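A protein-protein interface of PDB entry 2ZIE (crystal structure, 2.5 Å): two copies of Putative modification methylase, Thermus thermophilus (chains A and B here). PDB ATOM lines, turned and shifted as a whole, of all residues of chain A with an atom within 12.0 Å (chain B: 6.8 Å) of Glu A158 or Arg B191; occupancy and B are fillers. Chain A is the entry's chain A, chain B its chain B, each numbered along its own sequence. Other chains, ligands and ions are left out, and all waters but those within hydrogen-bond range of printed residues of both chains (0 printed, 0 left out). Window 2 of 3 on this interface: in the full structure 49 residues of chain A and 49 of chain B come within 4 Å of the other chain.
The backbone NH of Gly A160 sits at hydrogen-bond distance from the backbone carbonyl oxygen of Met B231, 2.8 Å away. The side-chain carboxylate of Glu A158 lies within salt-bridge range of the guanidinium group of Arg B191 (3.5 Å). The backbone carbonyl oxygen of Tyr A157 lies within hydrogen-bond range of the backbone NH of Leu B192 (2.8 Å). NH1 of Arg B187 is in salt-bridge range of OE2 of Glu A158 (3.1 Å).
The backbone carbonyl oxygen of Gln B186 lies within hydrogen-bond range of the side-chain hydroxyl of Ser B190 (2.8 Å). The guanidinium group (NH2) of Arg B187 lies close to the side-chain amide nitrogen (NE2) of Gln B184.
Tyr A157 touches Arg B191 (O to CG, 3.5 Å). Phe B197 touches Tyr A157. CD of Pro A159 touches O of Ser B190, at 3.5 Å. CG of Pro A159 touches O of Arg B230, 3.4 Å away. Pro A159 touches Met B231. CB of Ala A161 touches CZ of Phe B197 (3.6 Å). Ala A161 touches Phe B201 (O to CE2, 3.5 Å). Phe B201 touches Ile A163 (CD2 to CG1, 3.7 Å).
Printed residues of chain B within 4 Å of Tyr A157: Arg B191 (3.5 Å), Leu B192 (2.8 Å) and Phe B197 (3.4 Å). Of the printed residues of chain B, Pro A159 touches Ser B190 (3.5 Å), Arg B230 (3.4 Å) and Met B231 (3.2 Å). Printed residues of chain B within 4 Å of Gly A160: Met B231 (2.8 Å). Ile A162 touches none of the printed residues of chain B. No residue of chain A comes within 4 Å of Pro B182. Arg B187 touches just one residue of chain A: Glu A158. No residue of chain A comes within 4 Å of Glu B188. Of chain A, only Pro A159 (3.5 Å) comes within 4 Å of Ser B190. Of chain A, only Tyr A157 and Glu A158 come within 4 Å of Arg B191. Of the printed residues of chain A, Leu B192 touches Tyr A157. Pro B193 touches none of the printed residues of chain A. Printed residues of chain A within 4 Å of Met B231: Pro A159 and Gly A160. Arg B258 touches none of the printed residues of chain A. The nearest residue of chain A that does not touch Arg B191 is Pro A156 (4.6 Å). The nearest printed residue of chain A that does not touch Phe B197 is Glu A158 (4.3 Å).
Hydrophobic or aromatic side chains of chain B within 4 Å of the printed part of chain A: Leu B192, Phe B197 and Phe B201. Printed residues of chain A that touch a printed residue of chain B: Tyr A157, Glu A158, Pro A159, Gly A160, Ala A161 and Ile A163.
No position is printed for both chains.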
ATOM      1  N   PRO A 156      14.631 -33.853  18.693  1.00  0.00           N
ATOM      2  CA  PRO A 156      14.259 -32.440  18.534  1.00  0.00           C
ATOM      3  C   PRO A 156      15.370 -31.626  17.871  1.00  0.00           C
ATOM      4  O   PRO A 156      16.167 -32.158  17.099  1.00  0.00           O
ATOM      5  CB  PRO A 156      13.999 -31.995  19.967  1.00  0.00           C
ATOM      6  CG  PRO A 156      15.048 -32.777  20.724  1.00  0.00           C
ATOM      7  CD  PRO A 156      14.939 -34.160  20.103  1.00  0.00           C
ATOM      8  N   TYR A 157      15.411 -30.335  18.178  1.00  0.00           N
ATOM      9  CA  TYR A 157      16.433 -29.456  17.625  1.00  0.00           C
ATOM     10  C   TYR A 157      17.360 -29.055  18.757  1.00  0.00           C
ATOM     11  O   TYR A 157      17.479 -27.884  19.099  1.00  0.00           O
ATOM     12  CB  TYR A 157      15.782 -28.218  17.010  1.00  0.00           C
ATOM     13  CG  TYR A 157      14.809 -28.540  15.899  1.00  0.00           C
ATOM     14  CD1 TYR A 157      15.230 -29.208  14.752  1.00  0.00           C
ATOM     15  CD2 TYR A 157      13.465 -28.182  15.996  1.00  0.00           C
ATOM     16  CE1 TYR A 157      14.338 -29.512  13.729  1.00  0.00           C
ATOM     17  CE2 TYR A 157      12.567 -28.482  14.978  1.00  0.00           C
ATOM     18  CZ  TYR A 157      13.011 -29.145  13.850  1.00  0.00           C
ATOM     19  OH  TYR A 157      12.127 -29.444  12.838  1.00  0.00           O
ATOM     20  N   GLU A 158      18.019 -30.051  19.336  1.00  0.00           N
ATOM     21  CA  GLU A 158      18.916 -29.815  20.450  1.00  0.00           C
ATOM     22  C   GLU A 158      20.392 -30.027  20.133  1.00  0.00           C
ATOM     23  O   GLU A 158      20.750 -30.843  19.285  1.00  0.00           O
ATOM     24  CB  GLU A 158      18.472 -30.673  21.637  1.00  0.00           C
ATOM     25  CG  GLU A 158      17.280 -30.048  22.377  1.00  0.00           C
ATOM     26  CD  GLU A 158      16.576 -31.004  23.329  1.00  0.00           C
ATOM     27  OE1 GLU A 158      17.266 -31.628  24.165  1.00  0.00           O
ATOM     28  OE2 GLU A 158      15.326 -31.118  23.243  1.00  0.00           O
ATOM     29  N   PRO A 159      21.271 -29.278  20.818  1.00  0.00           N
ATOM     30  CA  PRO A 159      22.718 -29.367  20.619  1.00  0.00           C
ATOM     31  C   PRO A 159      23.201 -30.799  20.536  1.00  0.00           C
ATOM     32  O   PRO A 159      22.658 -31.671  21.196  1.00  0.00           O
ATOM     33  CB  PRO A 159      23.274 -28.643  21.840  1.00  0.00           C
ATOM     34  CG  PRO A 159      22.247 -27.591  22.087  1.00  0.00           C
ATOM     35  CD  PRO A 159      20.958 -28.358  21.928  1.00  0.00           C
ATOM     36  N   GLY A 160      24.211 -31.037  19.708  1.00  0.00           N
ATOM     37  CA  GLY A 160      24.779 -32.371  19.588  1.00  0.00           C
ATOM     38  C   GLY A 160      24.379 -33.192  18.385  1.00  0.00           C
ATOM     39  O   GLY A 160      24.908 -34.277  18.185  1.00  0.00           O
ATOM     40  N   ALA A 161      23.456 -32.684  17.575  1.00  0.00           N
ATOM     41  CA  ALA A 161      22.989 -33.413  16.396  1.00  0.00           C
ATOM     42  C   ALA A 161      24.126 -33.820  15.458  1.00  0.00           C
ATOM     43  O   ALA A 161      25.165 -33.173  15.394  1.00  0.00           O
ATOM     44  CB  ALA A 161      21.970 -32.574  15.644  1.00  0.00           C
ATOM     45  N   ILE A 162      23.925 -34.910  14.732  1.00  0.00           N
ATOM     46  CA  ILE A 162      24.929 -35.370  13.798  1.00  0.00           C
ATOM     47  C   ILE A 162      24.690 -34.735  12.449  1.00  0.00           C
ATOM     48  O   ILE A 162      23.562 -34.711  11.958  1.00  0.00           O
ATOM     49  CB  ILE A 162      24.893 -36.897  13.636  1.00  0.00           C
ATOM     50  CG1 ILE A 162      25.369 -37.549  14.927  1.00  0.00           C
ATOM     51  CG2 ILE A 162      25.786 -37.335  12.472  1.00  0.00           C
ATOM     52  CD1 ILE A 162      26.727 -37.037  15.402  1.00  0.00           C
ATOM     53  N   ILE A 163      25.750 -34.205  11.852  1.00  0.00           N
ATOM     54  CA  ILE A 163      25.621 -33.595  10.546  1.00  0.00           C
ATOM     55  C   ILE A 163      25.865 -34.654   9.479  1.00  0.00           C
ATOM     56  O   ILE A 163      26.909 -35.311   9.446  1.00  0.00           O
ATOM     57  CB  ILE A 163      26.599 -32.409  10.372  1.00  0.00           C
ATOM     58  CG1 ILE A 163      26.269 -31.327  11.403  1.00  0.00           C
ATOM     59  CG2 ILE A 163      26.475 -31.832   8.952  1.00  0.00           C
ATOM     60  CD1 ILE A 163      27.101 -30.079  11.292  1.00  0.00           C
ATOM     61  N   PRO B 182      21.940 -33.289  30.182  1.00  0.00           N
ATOM     62  CA  PRO B 182      21.665 -31.913  30.605  1.00  0.00           C
ATOM     63  C   PRO B 182      20.394 -31.792  31.445  1.00  0.00           C
ATOM     64  O   PRO B 182      19.496 -32.623  31.346  1.00  0.00           O
ATOM     65  CB  PRO B 182      21.542 -31.182  29.280  1.00  0.00           C
ATOM     66  CG  PRO B 182      20.831 -32.201  28.438  1.00  0.00           C
ATOM     67  CD  PRO B 182      21.537 -33.499  28.779  1.00  0.00           C
ATOM     68  N   GLN B 184      16.766 -30.210  32.637  1.00  0.00           N
ATOM     69  CA  GLN B 184      15.624 -29.840  31.836  1.00  0.00           C
ATOM     70  C   GLN B 184      15.686 -28.385  31.420  1.00  0.00           C
ATOM     71  O   GLN B 184      15.329 -28.045  30.295  1.00  0.00           O
ATOM     72  CB  GLN B 184      14.343 -30.095  32.615  1.00  0.00           C
ATOM     73  CG  GLN B 184      13.489 -31.209  32.045  1.00  0.00           C
ATOM     74  CD  GLN B 184      12.699 -30.763  30.842  1.00  0.00           C
ATOM     75  OE1 GLN B 184      12.057 -29.711  30.871  1.00  0.00           O
ATOM     76  NE2 GLN B 184      12.729 -31.561  29.780  1.00  0.00           N
ATOM     77  N   GLN B 186      18.313 -26.771  30.938  1.00  0.00           N
ATOM     78  CA  GLN B 186      19.413 -26.653  29.995  1.00  0.00           C
ATOM     79  C   GLN B 186      18.913 -27.012  28.608  1.00  0.00           C
ATOM     80  O   GLN B 186      19.270 -26.372  27.622  1.00  0.00           O
ATOM     81  CB  GLN B 186      20.570 -27.578  30.371  1.00  0.00           C
ATOM     82  CG  GLN B 186      21.496 -27.038  31.457  1.00  0.00           C
ATOM     83  CD  GLN B 186      22.666 -27.967  31.720  1.00  0.00           C
ATOM     84  OE1 GLN B 186      22.475 -29.131  32.068  1.00  0.00           O
ATOM     85  NE2 GLN B 186      23.889 -27.460  31.547  1.00  0.00           N
ATOM     86  N   ARG B 187      18.078 -28.042  28.537  1.00  0.00           N
ATOM     87  CA  ARG B 187      17.543 -28.468  27.261  1.00  0.00           C
ATOM     88  C   ARG B 187      16.639 -27.377  26.712  1.00  0.00           C
ATOM     89  O   ARG B 187      16.761 -26.972  25.560  1.00  0.00           O
ATOM     90  CB  ARG B 187      16.780 -29.780  27.428  1.00  0.00           C
ATOM     91  CG  ARG B 187      17.687 -30.948  27.776  1.00  0.00           C
ATOM     92  CD  ARG B 187      16.937 -32.249  28.088  1.00  0.00           C
ATOM     93  NE  ARG B 187      16.221 -32.816  26.944  1.00  0.00           N
ATOM     94  CZ  ARG B 187      15.013 -32.427  26.540  1.00  0.00           C
ATOM     95  NH1 ARG B 187      14.444 -33.001  25.488  1.00  0.00           N
ATOM     96  NH2 ARG B 187      14.368 -31.466  27.191  1.00  0.00           N
ATOM     97  N   GLU B 188      15.746 -26.884  27.552  1.00  0.00           N
ATOM     98  CA  GLU B 188      14.826 -25.844  27.141  1.00  0.00           C
ATOM     99  C   GLU B 188      15.531 -24.567  26.730  1.00  0.00           C
ATOM    100  O   GLU B 188      15.172 -23.956  25.731  1.00  0.00           O
ATOM    101  CB  GLU B 188      13.834 -25.541  28.263  1.00  0.00           C
ATOM    102  CG  GLU B 188      12.682 -26.526  28.330  1.00  0.00           C
ATOM    103  CD  GLU B 188      11.884 -26.407  29.617  1.00  0.00           C
ATOM    104  OE1 GLU B 188      10.798 -27.027  29.698  1.00  0.00           O
ATOM    105  OE2 GLU B 188      12.342 -25.702  30.549  1.00  0.00           O
ATOM    106  N   LYS B 189      16.538 -24.163  27.490  1.00  0.00           N
ATOM    107  CA  LYS B 189      17.243 -22.934  27.177  1.00  0.00           C
ATOM    108  C   LYS B 189      18.306 -23.071  26.100  1.00  0.00           C
ATOM    109  O   LYS B 189      18.888 -22.076  25.676  1.00  0.00           O
ATOM    110  CB  LYS B 189      17.858 -22.353  28.443  1.00  0.00           C
ATOM    111  CG  LYS B 189      16.840 -21.719  29.372  1.00  0.00           C
ATOM    112  CD  LYS B 189      17.519 -21.084  30.573  1.00  0.00           C
ATOM    113  CE  LYS B 189      16.504 -20.473  31.535  1.00  0.00           C
ATOM    114  NZ  LYS B 189      17.166 -19.877  32.736  1.00  0.00           N
ATOM    115  N   SER B 190      18.538 -24.294  25.643  1.00  0.00           N
ATOM    116  CA  SER B 190      19.543 -24.547  24.626  1.00  0.00           C
ATOM    117  C   SER B 190      18.958 -25.033  23.313  1.00  0.00           C
ATOM    118  O   SER B 190      19.663 -25.111  22.312  1.00  0.00           O
ATOM    119  CB  SER B 190      20.546 -25.577  25.135  1.00  0.00           C
ATOM    120  OG  SER B 190      21.279 -25.078  26.235  1.00  0.00           O
ATOM    121  N   ARG B 191      17.674 -25.376  23.317  1.00  0.00           N
ATOM    122  CA  ARG B 191      17.030 -25.851  22.105  1.00  0.00           C
ATOM    123  C   ARG B 191      17.168 -24.764  21.044  1.00  0.00           C
ATOM    124  O   ARG B 191      17.031 -23.581  21.331  1.00  0.00           O
ATOM    125  CB  ARG B 191      15.550 -26.168  22.368  1.00  0.00           C
ATOM    126  CG  ARG B 191      14.822 -26.824  21.185  1.00  0.00           C
ATOM    127  CD  ARG B 191      13.408 -27.298  21.544  1.00  0.00           C
ATOM    128  NE  ARG B 191      13.414 -28.300  22.617  1.00  0.00           N
ATOM    129  CZ  ARG B 191      12.887 -28.121  23.832  1.00  0.00           C
ATOM    130  NH1 ARG B 191      12.297 -26.974  24.151  1.00  0.00           N
ATOM    131  NH2 ARG B 191      12.964 -29.091  24.740  1.00  0.00           N
ATOM    132  N   LEU B 192      17.464 -25.169  19.822  1.00  0.00           N
ATOM    133  CA  LEU B 192      17.623 -24.218  18.742  1.00  0.00           C
ATOM    134  C   LEU B 192      16.339 -24.113  17.951  1.00  0.00           C
ATOM    135  O   LEU B 192      15.652 -25.114  17.736  1.00  0.00           O
ATOM    136  CB  LEU B 192      18.743 -24.666  17.808  1.00  0.00           C
ATOM    137  CG  LEU B 192      20.156 -24.608  18.370  1.00  0.00           C
ATOM    138  CD1 LEU B 192      21.067 -25.455  17.527  1.00  0.00           C
ATOM    139  CD2 LEU B 192      20.631 -23.165  18.395  1.00  0.00           C
ATOM    140  N   PRO B 193      15.987 -22.893  17.516  1.00  0.00           N
ATOM    141  CA  PRO B 193      14.766 -22.694  16.729  1.00  0.00           C
ATOM    142  C   PRO B 193      14.939 -23.500  15.449  1.00  0.00           C
ATOM    143  O   PRO B 193      16.057 -23.664  14.970  1.00  0.00           O
ATOM    144  CB  PRO B 193      14.768 -21.192  16.462  1.00  0.00           C
ATOM    145  CG  PRO B 193      15.489 -20.636  17.650  1.00  0.00           C
ATOM    146  CD  PRO B 193      16.636 -21.606  17.814  1.00  0.00           C
ATOM    147  N   PHE B 197      18.569 -24.218  13.452  1.00  0.00           N
ATOM    148  CA  PHE B 197      19.011 -25.599  13.394  1.00  0.00           C
ATOM    149  C   PHE B 197      19.385 -26.036  11.987  1.00  0.00           C
ATOM    150  O   PHE B 197      20.433 -26.628  11.781  1.00  0.00           O
ATOM    151  CB  PHE B 197      17.930 -26.535  13.919  1.00  0.00           C
ATOM    152  CG  PHE B 197      18.390 -27.954  14.074  1.00  0.00           C
ATOM    153  CD1 PHE B 197      19.058 -28.361  15.230  1.00  0.00           C
ATOM    154  CD2 PHE B 197      18.199 -28.873  13.051  1.00  0.00           C
ATOM    155  CE1 PHE B 197      19.531 -29.660  15.367  1.00  0.00           C
ATOM    156  CE2 PHE B 197      18.669 -30.176  13.174  1.00  0.00           C
ATOM    157  CZ  PHE B 197      19.339 -30.571  14.337  1.00  0.00           C
ATOM    158  N   PHE B 201      23.273 -26.897  11.212  1.00  0.00           N
ATOM    159  CA  PHE B 201      23.676 -28.272  11.010  1.00  0.00           C
ATOM    160  C   PHE B 201      23.741 -28.730   9.570  1.00  0.00           C
ATOM    161  O   PHE B 201      22.982 -29.590   9.146  1.00  0.00           O
ATOM    162  CB  PHE B 201      22.775 -29.210  11.811  1.00  0.00           C
ATOM    163  CG  PHE B 201      22.977 -29.121  13.290  1.00  0.00           C
ATOM    164  CD1 PHE B 201      22.297 -28.174  14.042  1.00  0.00           C
ATOM    165  CD2 PHE B 201      23.895 -29.955  13.928  1.00  0.00           C
ATOM    166  CE1 PHE B 201      22.529 -28.054  15.409  1.00  0.00           C
ATOM    167  CE2 PHE B 201      24.134 -29.839  15.294  1.00  0.00           C
ATOM    168  CZ  PHE B 201      23.450 -28.886  16.035  1.00  0.00           C
ATOM    169  N   ARG B 230      26.516 -22.741  20.382  1.00  0.00           N
ATOM    170  CA  ARG B 230      25.106 -23.093  20.464  1.00  0.00           C
ATOM    171  C   ARG B 230      24.797 -24.505  19.999  1.00  0.00           C
ATOM    172  O   ARG B 230      23.806 -25.087  20.414  1.00  0.00           O
ATOM    173  CB  ARG B 230      24.261 -22.102  19.659  1.00  0.00           C
ATOM    174  CG  ARG B 230      24.391 -20.669  20.122  1.00  0.00           C
ATOM    175  CD  ARG B 230      23.608 -19.751  19.222  1.00  0.00           C
ATOM    176  NE  ARG B 230      22.177 -20.003  19.307  1.00  0.00           N
ATOM    177  CZ  ARG B 230      21.277 -19.507  18.469  1.00  0.00           C
ATOM    178  NH1 ARG B 230      21.657 -18.726  17.471  1.00  0.00           N
ATOM    179  NH2 ARG B 230      19.999 -19.797  18.627  1.00  0.00           N
ATOM    180  N   MET B 231      25.657 -25.064  19.160  1.00  0.00           N
ATOM    181  CA  MET B 231      25.435 -26.401  18.626  1.00  0.00           C
ATOM    182  C   MET B 231      26.028 -27.540  19.420  1.00  0.00           C
ATOM    183  O   MET B 231      25.567 -28.676  19.314  1.00  0.00           O
ATOM    184  CB  MET B 231      26.009 -26.500  17.219  1.00  0.00           C
ATOM    185  CG  MET B 231      25.557 -25.430  16.293  1.00  0.00           C
ATOM    186  SD  MET B 231      26.554 -25.647  14.603  1.00  0.00           S
ATOM    187  CE  MET B 231      28.384 -25.399  15.261  1.00  0.00           C
ATOM    188  N   PHE B 234      25.542 -26.635  26.219  1.00  0.00           N
ATOM    189  CA  PHE B 234      24.286 -26.179  26.791  1.00  0.00           C
ATOM    190  C   PHE B 234      24.596 -24.978  27.623  1.00  0.00           C
ATOM    191  O   PHE B 234      25.743 -24.782  28.012  1.00  0.00           O
ATOM    192  CB  PHE B 234      23.680 -27.250  27.688  1.00  0.00           C
ATOM    193  CG  PHE B 234      23.306 -28.496  26.964  1.00  0.00           C
ATOM    194  CD1 PHE B 234      22.068 -28.604  26.336  1.00  0.00           C
ATOM    195  CD2 PHE B 234      24.195 -29.560  26.889  1.00  0.00           C
ATOM    196  CE1 PHE B 234      21.718 -29.747  25.643  1.00  0.00           C
ATOM    197  CE2 PHE B 234      23.858 -30.716  26.198  1.00  0.00           C
ATOM    198  CZ  PHE B 234      22.614 -30.811  25.571  1.00  0.00           C
ATOM    199  N   ARG B 258      27.276 -19.470  28.442  1.00  0.00           N
ATOM    200  CA  ARG B 258      28.167 -20.583  28.751  1.00  0.00           C
ATOM    201  C   ARG B 258      29.323 -19.994  29.554  1.00  0.00           C
ATOM    202  O   ARG B 258      29.599 -18.800  29.464  1.00  0.00           O
ATOM    203  CB  ARG B 258      28.707 -21.239  27.482  1.00  0.00           C
ATOM    204  CG  ARG B 258      27.844 -22.349  26.923  1.00  0.00           C
ATOM    205  CD  ARG B 258      26.566 -21.820  26.319  1.00  0.00           C
ATOM    206  NE  ARG B 258      25.895 -22.830  25.502  1.00  0.00           N
ATOM    207  CZ  ARG B 258      24.693 -22.670  24.953  1.00  0.00           C
ATOM    208  NH1 ARG B 258      24.025 -21.532  25.136  1.00  0.00           N
ATOM    209  NH2 ARG B 258      24.160 -23.639  24.220  1.00  0.00           N
